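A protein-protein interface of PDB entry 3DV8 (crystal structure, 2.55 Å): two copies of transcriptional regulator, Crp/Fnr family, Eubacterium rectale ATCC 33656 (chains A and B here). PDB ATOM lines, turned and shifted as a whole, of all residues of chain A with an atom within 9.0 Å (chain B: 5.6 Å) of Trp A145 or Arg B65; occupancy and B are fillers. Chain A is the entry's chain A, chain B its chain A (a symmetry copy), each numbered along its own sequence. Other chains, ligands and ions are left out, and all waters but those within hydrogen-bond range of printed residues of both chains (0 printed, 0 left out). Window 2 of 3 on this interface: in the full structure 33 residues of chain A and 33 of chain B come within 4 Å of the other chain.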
ATOM      1  N   MET A 137     -21.993 -31.703  -0.085  1.00  0.00           N
ATOM      2  CA  MET A 137     -23.144 -31.584   0.849  1.00  0.00           C
ATOM      3  C   MET A 137     -23.195 -30.242   1.577  1.00  0.00           C
ATOM      4  O   MET A 137     -24.295 -29.766   1.877  1.00  0.00           O
ATOM      5  CB  MET A 137     -23.199 -32.754   1.824  1.00  0.00           C
ATOM      6  CG  MET A 137     -23.562 -34.077   1.168  1.00  0.00           C
ATOM      7  SD  MET A 137     -25.440 -34.221   0.742  1.00  0.00           S
ATOM      8  CE  MET A 137     -25.458 -33.226  -0.741  1.00  0.00           C
ATOM      9  N   TRP A 138     -22.026 -29.658   1.876  1.00  0.00           N
ATOM     10  CA  TRP A 138     -21.956 -28.300   2.427  1.00  0.00           C
ATOM     11  C   TRP A 138     -22.487 -27.311   1.375  1.00  0.00           C
ATOM     12  O   TRP A 138     -23.178 -26.345   1.735  1.00  0.00           O
ATOM     13  CB  TRP A 138     -20.541 -27.917   2.889  1.00  0.00           C
ATOM     14  CG  TRP A 138     -20.387 -26.436   3.157  1.00  0.00           C
ATOM     15  CD1 TRP A 138     -20.797 -25.747   4.271  1.00  0.00           C
ATOM     16  CD2 TRP A 138     -19.805 -25.459   2.270  1.00  0.00           C
ATOM     17  NE1 TRP A 138     -20.501 -24.403   4.133  1.00  0.00           N
ATOM     18  CE2 TRP A 138     -19.894 -24.199   2.919  1.00  0.00           C
ATOM     19  CE3 TRP A 138     -19.213 -25.529   0.989  1.00  0.00           C
ATOM     20  CZ2 TRP A 138     -19.403 -23.012   2.329  1.00  0.00           C
ATOM     21  CZ3 TRP A 138     -18.730 -24.347   0.394  1.00  0.00           C
ATOM     22  CH2 TRP A 138     -18.829 -23.105   1.071  1.00  0.00           C
ATOM     23  N   LEU A 139     -22.168 -27.572   0.096  1.00  0.00           N
ATOM     24  CA  LEU A 139     -22.656 -26.767  -1.017  1.00  0.00           C
ATOM     25  C   LEU A 139     -24.186 -26.828  -1.147  1.00  0.00           C
ATOM     26  O   LEU A 139     -24.795 -25.778  -1.338  1.00  0.00           O
ATOM     27  CB  LEU A 139     -21.972 -27.147  -2.334  1.00  0.00           C
ATOM     28  CG  LEU A 139     -22.284 -26.290  -3.571  1.00  0.00           C
ATOM     29  CD1 LEU A 139     -22.035 -24.822  -3.330  1.00  0.00           C
ATOM     30  CD2 LEU A 139     -21.468 -26.761  -4.729  1.00  0.00           C
ATOM     31  N   ILE A 140     -24.804 -28.017  -1.043  1.00  0.00           N
ATOM     32  CA  ILE A 140     -26.289 -28.111  -1.093  1.00  0.00           C
ATOM     33  C   ILE A 140     -26.894 -27.294   0.053  1.00  0.00           C
ATOM     34  O   ILE A 140     -27.800 -26.499  -0.182  1.00  0.00           O
ATOM     35  CB  ILE A 140     -26.864 -29.566  -1.069  1.00  0.00           C
ATOM     36  CG1 ILE A 140     -26.563 -30.291  -2.383  1.00  0.00           C
ATOM     37  CG2 ILE A 140     -28.391 -29.566  -0.860  1.00  0.00           C
ATOM     38  CD1 ILE A 140     -27.461 -31.548  -2.646  1.00  0.00           C
ATOM     39  N   GLU A 141     -26.352 -27.479   1.263  1.00  0.00           N
ATOM     40  CA  GLU A 141     -26.772 -26.727   2.460  1.00  0.00           C
ATOM     41  C   GLU A 141     -26.647 -25.205   2.272  1.00  0.00           C
ATOM     42  O   GLU A 141     -27.556 -24.470   2.690  1.00  0.00           O
ATOM     43  CB  GLU A 141     -26.005 -27.200   3.715  1.00  0.00           C
ATOM     44  CG  GLU A 141     -26.406 -28.632   4.174  1.00  0.00           C
ATOM     45  CD  GLU A 141     -25.482 -29.271   5.232  1.00  0.00           C
ATOM     46  OE1 GLU A 141     -24.497 -28.639   5.678  1.00  0.00           O
ATOM     47  OE2 GLU A 141     -25.751 -30.437   5.616  1.00  0.00           O
ATOM     48  N   GLN A 142     -25.562 -24.763   1.604  1.00  0.00           N
ATOM     49  CA  GLN A 142     -25.322 -23.336   1.346  1.00  0.00           C
ATOM     50  C   GLN A 142     -26.335 -22.825   0.307  1.00  0.00           C
ATOM     51  O   GLN A 142     -27.004 -21.821   0.538  1.00  0.00           O
ATOM     52  CB  GLN A 142     -23.875 -23.046   0.878  1.00  0.00           C
ATOM     53  CG  GLN A 142     -23.454 -21.582   1.106  1.00  0.00           C
ATOM     54  CD  GLN A 142     -22.209 -21.110   0.321  1.00  0.00           C
ATOM     55  OE1 GLN A 142     -22.136 -21.223  -0.907  1.00  0.00           O
ATOM     56  NE2 GLN A 142     -21.262 -20.511   1.038  1.00  0.00           N
ATOM     57  N   ILE A 143     -26.458 -23.529  -0.824  1.00  0.00           N
ATOM     58  CA  ILE A 143     -27.396 -23.174  -1.920  1.00  0.00           C
ATOM     59  C   ILE A 143     -28.861 -23.059  -1.470  1.00  0.00           C
ATOM     60  O   ILE A 143     -29.555 -22.106  -1.831  1.00  0.00           O
ATOM     61  CB  ILE A 143     -27.352 -24.222  -3.069  1.00  0.00           C
ATOM     62  CG1 ILE A 143     -26.033 -24.153  -3.835  1.00  0.00           C
ATOM     63  CG2 ILE A 143     -28.467 -24.002  -4.073  1.00  0.00           C
ATOM     64  CD1 ILE A 143     -25.800 -25.385  -4.689  1.00  0.00           C
ATOM     65  N   MET A 144     -29.312 -24.034  -0.686  1.00  0.00           N
ATOM     66  CA  MET A 144     -30.707 -24.107  -0.229  1.00  0.00           C
ATOM     67  C   MET A 144     -31.064 -23.142   0.890  1.00  0.00           C
ATOM     68  O   MET A 144     -32.036 -22.387   0.777  1.00  0.00           O
ATOM     69  CB  MET A 144     -31.030 -25.534   0.240  1.00  0.00           C
ATOM     70  CG  MET A 144     -30.946 -26.609  -0.828  1.00  0.00           C
ATOM     71  SD  MET A 144     -32.388 -26.560  -2.098  1.00  0.00           S
ATOM     72  CE  MET A 144     -31.962 -25.042  -3.193  1.00  0.00           C
ATOM     73  N   TRP A 145     -30.261 -23.165   1.951  1.00  0.00           N
ATOM     74  CA  TRP A 145     -30.568 -22.420   3.171  1.00  0.00           C
ATOM     75  C   TRP A 145     -30.050 -20.971   3.219  1.00  0.00           C
ATOM     76  O   TRP A 145     -30.643 -20.152   3.926  1.00  0.00           O
ATOM     77  CB  TRP A 145     -30.135 -23.218   4.423  1.00  0.00           C
ATOM     78  CG  TRP A 145     -30.487 -24.734   4.417  1.00  0.00           C
ATOM     79  CD1 TRP A 145     -29.667 -25.760   4.832  1.00  0.00           C
ATOM     80  CD2 TRP A 145     -31.687 -25.370   3.910  1.00  0.00           C
ATOM     81  NE1 TRP A 145     -30.297 -26.980   4.663  1.00  0.00           N
ATOM     82  CE2 TRP A 145     -31.528 -26.776   4.095  1.00  0.00           C
ATOM     83  CE3 TRP A 145     -32.886 -24.893   3.333  1.00  0.00           C
ATOM     84  CZ2 TRP A 145     -32.524 -27.709   3.730  1.00  0.00           C
ATOM     85  CZ3 TRP A 145     -33.882 -25.827   2.964  1.00  0.00           C
ATOM     86  CH2 TRP A 145     -33.684 -27.217   3.166  1.00  0.00           C
ATOM     87  N   LYS A 146     -28.991 -20.637   2.477  1.00  0.00           N
ATOM     88  CA  LYS A 146     -28.437 -19.271   2.482  1.00  0.00           C
ATOM     89  C   LYS A 146     -28.721 -18.469   1.201  1.00  0.00           C
ATOM     90  O   LYS A 146     -28.454 -18.932   0.100  1.00  0.00           O
ATOM     91  CB  LYS A 146     -26.946 -19.310   2.850  1.00  0.00           C
ATOM     92  CG  LYS A 146     -26.754 -19.694   4.347  1.00  0.00           C
ATOM     93  CD  LYS A 146     -25.297 -19.689   4.819  1.00  0.00           C
ATOM     94  CE  LYS A 146     -25.192 -19.753   6.356  1.00  0.00           C
ATOM     95  NZ  LYS A 146     -25.703 -18.506   7.043  1.00  0.00           N
ATOM     96  N   SER A 147     -29.292 -17.269   1.372  1.00  0.00           N
ATOM     97  CA  SER A 147     -29.590 -16.332   0.269  1.00  0.00           C
ATOM     98  C   SER A 147     -28.313 -15.808  -0.415  1.00  0.00           C
ATOM     99  O   SER A 147     -27.226 -15.857   0.164  1.00  0.00           O
ATOM    100  CB  SER A 147     -30.446 -15.167   0.772  1.00  0.00           C
ATOM    101  OG  SER A 147     -29.871 -14.596   1.928  1.00  0.00           O
ATOM    102  N   LEU A 148     -28.477 -15.282  -1.634  1.00  0.00           N
ATOM    103  CA  LEU A 148     -27.353 -14.876  -2.504  1.00  0.00           C
ATOM    104  C   LEU A 148     -26.424 -13.830  -1.885  1.00  0.00           C
ATOM    105  O   LEU A 148     -25.209 -13.942  -2.042  1.00  0.00           O
ATOM    106  CB  LEU A 148     -27.840 -14.444  -3.897  1.00  0.00           C
ATOM    107  CG  LEU A 148     -26.796 -14.245  -5.010  1.00  0.00           C
ATOM    108  CD1 LEU A 148     -25.963 -15.494  -5.297  1.00  0.00           C
ATOM    109  CD2 LEU A 148     -27.496 -13.787  -6.280  1.00  0.00           C
ATOM    110  N   ASP A 149     -26.986 -12.843  -1.183  1.00  0.00           N
ATOM    111  CA  ASP A 149     -26.182 -11.833  -0.464  1.00  0.00           C
ATOM    112  C   ASP A 149     -25.211 -12.496   0.536  1.00  0.00           C
ATOM    113  O   ASP A 149     -24.039 -12.113   0.609  1.00  0.00           O
ATOM    114  CB  ASP A 149     -27.053 -10.750   0.236  1.00  0.00           C
ATOM    115  CG  ASP A 149     -28.027 -11.315   1.284  1.00  0.00           C
ATOM    116  OD1 ASP A 149     -28.511 -12.456   1.125  1.00  0.00           O
ATOM    117  OD2 ASP A 149     -28.329 -10.595   2.258  1.00  0.00           O
ATOM    118  N   LYS A 150     -25.689 -13.515   1.255  1.00  0.00           N
ATOM    119  CA  LYS A 150     -24.860 -14.236   2.227  1.00  0.00           C
ATOM    120  C   LYS A 150     -23.769 -15.069   1.563  1.00  0.00           C
ATOM    121  O   LYS A 150     -22.642 -15.126   2.059  1.00  0.00           O
ATOM    122  CB  LYS A 150     -25.722 -15.098   3.153  1.00  0.00           C
ATOM    123  CG  LYS A 150     -26.658 -14.265   4.003  1.00  0.00           C
ATOM    124  CD  LYS A 150     -27.264 -15.033   5.159  1.00  0.00           C
ATOM    125  CE  LYS A 150     -28.666 -15.510   4.912  1.00  0.00           C
ATOM    126  NZ  LYS A 150     -29.684 -14.399   5.019  1.00  0.00           N
ATOM    127  N   ARG A 151     -24.100 -15.668   0.422  1.00  0.00           N
ATOM    128  CA  ARG A 151     -23.161 -16.500  -0.341  1.00  0.00           C
ATOM    129  C   ARG A 151     -22.073 -15.669  -1.022  1.00  0.00           C
ATOM    130  O   ARG A 151     -20.929 -16.114  -1.090  1.00  0.00           O
ATOM    131  CB  ARG A 151     -23.917 -17.384  -1.340  1.00  0.00           C
ATOM    132  CG  ARG A 151     -24.859 -18.353  -0.620  1.00  0.00           C
ATOM    133  CD  ARG A 151     -25.672 -19.225  -1.529  1.00  0.00           C
ATOM    134  NE  ARG A 151     -24.815 -20.072  -2.353  1.00  0.00           N
ATOM    135  CZ  ARG A 151     -24.808 -20.162  -3.689  1.00  0.00           C
ATOM    136  NH1 ARG A 151     -25.698 -19.538  -4.466  1.00  0.00           N
ATOM    137  NH2 ARG A 151     -23.915 -20.980  -4.253  1.00  0.00           N
ATOM    138  N   GLN A 218     -22.570 -13.517   6.115  1.00  0.00           N
ATOM    139  CA  GLN A 218     -22.257 -14.956   5.969  1.00  0.00           C
ATOM    140  C   GLN A 218     -22.923 -15.807   7.070  1.00  0.00           C
ATOM    141  O   GLN A 218     -23.560 -16.826   6.791  1.00  0.00           O
ATOM    142  CB  GLN A 218     -20.729 -15.148   6.029  1.00  0.00           C
ATOM    143  CG  GLN A 218     -20.187 -16.590   5.966  1.00  0.00           C
ATOM    144  CD  GLN A 218     -18.692 -16.659   6.258  1.00  0.00           C
ATOM    145  OE1 GLN A 218     -18.215 -16.119   7.265  1.00  0.00           O
ATOM    146  NE2 GLN A 218     -17.947 -17.347   5.391  1.00  0.00           N
ATOM    147  N   ARG A 219     -22.772 -15.343   8.310  1.00  0.00           N
ATOM    148  CA  ARG A 219     -23.292 -16.014   9.497  1.00  0.00           C
ATOM    149  C   ARG A 219     -24.808 -15.871   9.667  1.00  0.00           C
ATOM    150  O   ARG A 219     -25.412 -16.776  10.226  1.00  0.00           O
ATOM    151  CB  ARG A 219     -22.591 -15.490  10.754  1.00  0.00           C
ATOM    152  CG  ARG A 219     -21.077 -15.672  10.768  1.00  0.00           C
ATOM    153  CD  ARG A 219     -20.618 -17.009  11.235  1.00  0.00           C
ATOM    154  NE  ARG A 219     -19.167 -17.126  11.060  1.00  0.00           N
ATOM    155  CZ  ARG A 219     -18.408 -18.127  11.514  1.00  0.00           C
ATOM    156  NH1 ARG A 219     -18.930 -19.135  12.227  1.00  0.00           N
ATOM    157  NH2 ARG A 219     -17.093 -18.111  11.265  1.00  0.00           N
ATOM    158  N   SER A 220     -25.411 -14.762   9.207  1.00  0.00           N
ATOM    159  CA  SER A 220     -26.878 -14.525   9.315  1.00  0.00           C
ATOM    160  C   SER A 220     -27.774 -15.653   8.767  1.00  0.00           C
ATOM    161  O   SER A 220     -27.388 -16.496   7.944  1.00  0.00           O
ATOM    162  CB  SER A 220     -27.296 -13.205   8.638  1.00  0.00           C
ATOM    163  OG  SER A 220     -26.766 -12.087   9.300  1.00  0.00           O
ATOM    164  OXT SER A 220     -28.937 -15.735   9.175  1.00  0.00           O
ATOM    165  N   ILE B  59     -32.343 -34.019   4.340  1.00  0.00           N
ATOM    166  CA  ILE B  59     -31.643 -33.120   5.245  1.00  0.00           C
ATOM    167  C   ILE B  59     -32.630 -32.079   5.745  1.00  0.00           C
ATOM    168  O   ILE B  59     -33.582 -31.743   5.051  1.00  0.00           O
ATOM    169  CB  ILE B  59     -30.361 -32.510   4.610  1.00  0.00           C
ATOM    170  CG1 ILE B  59     -30.660 -31.676   3.349  1.00  0.00           C
ATOM    171  CG2 ILE B  59     -29.372 -33.635   4.304  1.00  0.00           C
ATOM    172  CD1 ILE B  59     -29.437 -30.979   2.778  1.00  0.00           C
ATOM    173  N   LEU B  60     -32.392 -31.606   6.964  1.00  0.00           N
ATOM    174  CA  LEU B  60     -33.226 -30.630   7.647  1.00  0.00           C
ATOM    175  C   LEU B  60     -32.410 -29.384   7.955  1.00  0.00           C
ATOM    176  O   LEU B  60     -31.288 -29.497   8.451  1.00  0.00           O
ATOM    177  CB  LEU B  60     -33.750 -31.224   8.971  1.00  0.00           C
ATOM    178  CG  LEU B  60     -35.081 -31.981   8.983  1.00  0.00           C
ATOM    179  CD1 LEU B  60     -35.139 -32.944  10.154  1.00  0.00           C
ATOM    180  CD2 LEU B  60     -36.252 -30.996   9.034  1.00  0.00           C
ATOM    181  N   SER B  61     -32.970 -28.209   7.671  1.00  0.00           N
ATOM    182  CA  SER B  61     -32.341 -26.950   8.069  1.00  0.00           C
ATOM    183  C   SER B  61     -32.660 -26.778   9.553  1.00  0.00           C
ATOM    184  O   SER B  61     -33.596 -27.410  10.085  1.00  0.00           O
ATOM    185  CB  SER B  61     -32.878 -25.735   7.285  1.00  0.00           C
ATOM    186  OG  SER B  61     -34.095 -25.209   7.803  1.00  0.00           O
ATOM    187  N   GLU B  63     -34.197 -24.408  10.797  1.00  0.00           N
ATOM    188  CA  GLU B  63     -35.568 -23.878  10.813  1.00  0.00           C
ATOM    189  C   GLU B  63     -36.643 -24.909  10.382  1.00  0.00           C
ATOM    190  O   GLU B  63     -37.792 -24.522  10.137  1.00  0.00           O
ATOM    191  CB  GLU B  63     -35.658 -22.674   9.871  1.00  0.00           C
ATOM    192  CG  GLU B  63     -34.651 -21.565  10.146  1.00  0.00           C
ATOM    193  CD  GLU B  63     -34.858 -20.349   9.253  1.00  0.00           C
ATOM    194  OE1 GLU B  63     -35.381 -20.507   8.119  1.00  0.00           O
ATOM    195  OE2 GLU B  63     -34.485 -19.233   9.690  1.00  0.00           O
ATOM    196  N   GLY B  64     -36.288 -26.197  10.269  1.00  0.00           N
ATOM    197  CA  GLY B  64     -37.241 -27.256   9.871  1.00  0.00           C
ATOM    198  C   GLY B  64     -37.579 -27.430   8.390  1.00  0.00           C
ATOM    199  O   GLY B  64     -38.493 -28.183   8.052  1.00  0.00           O
ATOM    200  N   ARG B  65     -36.851 -26.745   7.504  1.00  0.00           N
ATOM    201  CA  ARG B  65     -37.035 -26.875   6.042  1.00  0.00           C
ATOM    202  C   ARG B  65     -36.367 -28.175   5.621  1.00  0.00           C
ATOM    203  O   ARG B  65     -35.353 -28.555   6.206  1.00  0.00           O
ATOM    204  CB  ARG B  65     -36.356 -25.729   5.308  1.00  0.00           C
ATOM    205  CG  ARG B  65     -36.890 -24.342   5.639  1.00  0.00           C
ATOM    206  CD  ARG B  65     -38.238 -24.039   4.991  1.00  0.00           C
ATOM    207  NE  ARG B  65     -38.162 -24.211   3.543  1.00  0.00           N
ATOM    208  CZ  ARG B  65     -37.512 -23.404   2.690  1.00  0.00           C
ATOM    209  NH1 ARG B  65     -36.850 -22.307   3.089  1.00  0.00           N
ATOM    210  NH2 ARG B  65     -37.526 -23.702   1.395  1.00  0.00           N
ATOM    211  N   GLU B  66     -36.912 -28.837   4.605  1.00  0.00           N
ATOM    212  CA  GLU B  66     -36.406 -30.134   4.153  1.00  0.00           C
ATOM    213  C   GLU B  66     -36.246 -30.230   2.644  1.00  0.00           C
ATOM    214  O   GLU B  66     -36.969 -29.568   1.919  1.00  0.00           O
ATOM    215  CB  GLU B  66     -37.396 -31.243   4.560  1.00  0.00           C
ATOM    216  CG  GLU B  66     -37.555 -31.491   6.048  1.00  0.00           C
ATOM    217  CD  GLU B  66     -38.629 -32.536   6.392  1.00  0.00           C
ATOM    218  OE1 GLU B  66     -39.062 -33.291   5.521  1.00  0.00           O
ATOM    219  OE2 GLU B  66     -39.052 -32.609   7.556  1.00  0.00           O
ATOM    220  N   ILE B  67     -35.321 -31.084   2.193  1.00  0.00           N
ATOM    221  CA  ILE B  67     -35.177 -31.466   0.770  1.00  0.00           C
ATOM    222  C   ILE B  67     -34.709 -32.937   0.713  1.00  0.00           C
ATOM    223  O   ILE B  67     -33.785 -33.310   1.430  1.00  0.00           O
ATOM    224  CB  ILE B  67     -34.262 -30.504  -0.066  1.00  0.00           C
ATOM    225  CG1 ILE B  67     -34.320 -30.863  -1.563  1.00  0.00           C
ATOM    226  CG2 ILE B  67     -32.826 -30.505   0.426  1.00  0.00           C
ATOM    227  CD1 ILE B  67     -33.582 -29.885  -2.486  1.00  0.00           C
ATOM    228  N   ASN B 177     -41.457 -30.317   1.201  1.00  0.00           N
ATOM    229  CA  ASN B 177     -40.383 -31.032   1.910  1.00  0.00           C
ATOM    230  C   ASN B 177     -39.518 -31.907   0.995  1.00  0.00           C
ATOM    231  O   ASN B 177     -38.345 -32.118   1.282  1.00  0.00           O
ATOM    232  CB  ASN B 177     -40.945 -31.856   3.080  1.00  0.00           C
ATOM    233  CG  ASN B 177     -41.537 -30.983   4.203  1.00  0.00           C
ATOM    234  OD1 ASN B 177     -41.341 -29.766   4.236  1.00  0.00           O
ATOM    235  ND2 ASN B 177     -42.268 -31.610   5.120  1.00  0.00           N
ATOM    236  N   GLY B 180     -37.416 -28.852  -1.192  1.00  0.00           N
ATOM    237  CA  GLY B 180     -36.732 -27.722  -0.556  1.00  0.00           C
ATOM    238  C   GLY B 180     -37.452 -26.399  -0.767  1.00  0.00           C
ATOM    239  O   GLY B 180     -36.797 -25.359  -0.827  1.00  0.00           O
ATOM    240  N   SER B 181     -38.787 -26.430  -0.858  1.00  0.00           N
ATOM    241  CA  SER B 181     -39.622 -25.236  -1.053  1.00  0.00           C
ATOM    242  C   SER B 181     -40.530 -25.018   0.170  1.00  0.00           C
ATOM    243  O   SER B 181     -40.400 -25.732   1.174  1.00  0.00           O
ATOM    244  CB  SER B 181     -40.447 -25.398  -2.331  1.00  0.00           C
ATOM    245  OG  SER B 181     -41.095 -24.181  -2.664  1.00  0.00           O
ATOM    246  N   HIS B 182     -41.383 -23.990   0.108  1.00  0.00           N
ATOM    247  CA  HIS B 182     -42.374 -23.690   1.163  1.00  0.00           C
ATOM    248  C   HIS B 182     -43.754 -24.101   0.650  1.00  0.00           C
ATOM    249  O   HIS B 182     -44.012 -23.990  -0.545  1.00  0.00           O
ATOM    250  CB  HIS B 182     -42.341 -22.203   1.546  1.00  0.00           C
ATOM    251  CG  HIS B 182     -43.221 -21.842   2.709  1.00  0.00           C
ATOM    252  ND1 HIS B 182     -44.455 -21.242   2.555  1.00  0.00           N
ATOM    253  CD2 HIS B 182     -43.034 -21.978   4.045  1.00  0.00           C
ATOM    254  CE1 HIS B 182     -44.993 -21.036   3.745  1.00  0.00           C
ATOM    255  NE2 HIS B 182     -44.150 -21.472   4.665  1.00  0.00           N
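N of Ile B67 sits close to O of Asn B177 (3.3 Å). The guanidinium group (NH2) of Arg B65 lies within hydrogen-bond range of the backbone carbonyl oxygen (O) of Gly B180 (2.9 Å). OG of Ser B61 sits at hydrogen-bond distance from N of Arg B65, 3.2 Å away. O of Glu B66 lies close to N of Gly B180 (3.2 Å). The backbone NH (N) of Glu B63 lies close to the side-chain hydroxyl (OG) of Ser B61, 3.1 Å away. OG of Ser B61 is in hydrogen-bond range of N of Gly B64 (3.4 Å).
Among the printed residues, pairs that only touch across the chains: Met A144 with Ile B67, Trp A145 with Ser B61, Trp A145 with Arg B65 and Trp A145 with Glu B66.
Of the printed residues of chain B, Met A144 touches Ile B67. Of the printed residues of chain B, Trp A145 touches Ser B61, Arg B65 and Glu B66. Leu A148 touches none of the printed residues of chain B. Of the printed residues of chain A, Ser B61 touches Trp A145 (3.6 Å). No residue of chain A comes within 4 Å of Gly B64. Of the printed residues of chain A, Glu B66 touches Trp A145 (3.9 Å). Of the printed residues of chain A, Ile B67 touches Met A144. His B182 touches none of the printed residues of chain A. The nearest printed residue of chain B that does not touch Met A144 is Gly B180 (4.7 Å).
Printed residues of chain B that touch a printed residue of chain A: Ser B61, Arg B65, Glu B66 and Ile B67. Hydrophobic or aromatic side chains of chain B that line the printed part of chain A: Ile B67. Among the printed residues, 4 pairs touch across the chains.
No position is printed for both chains.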
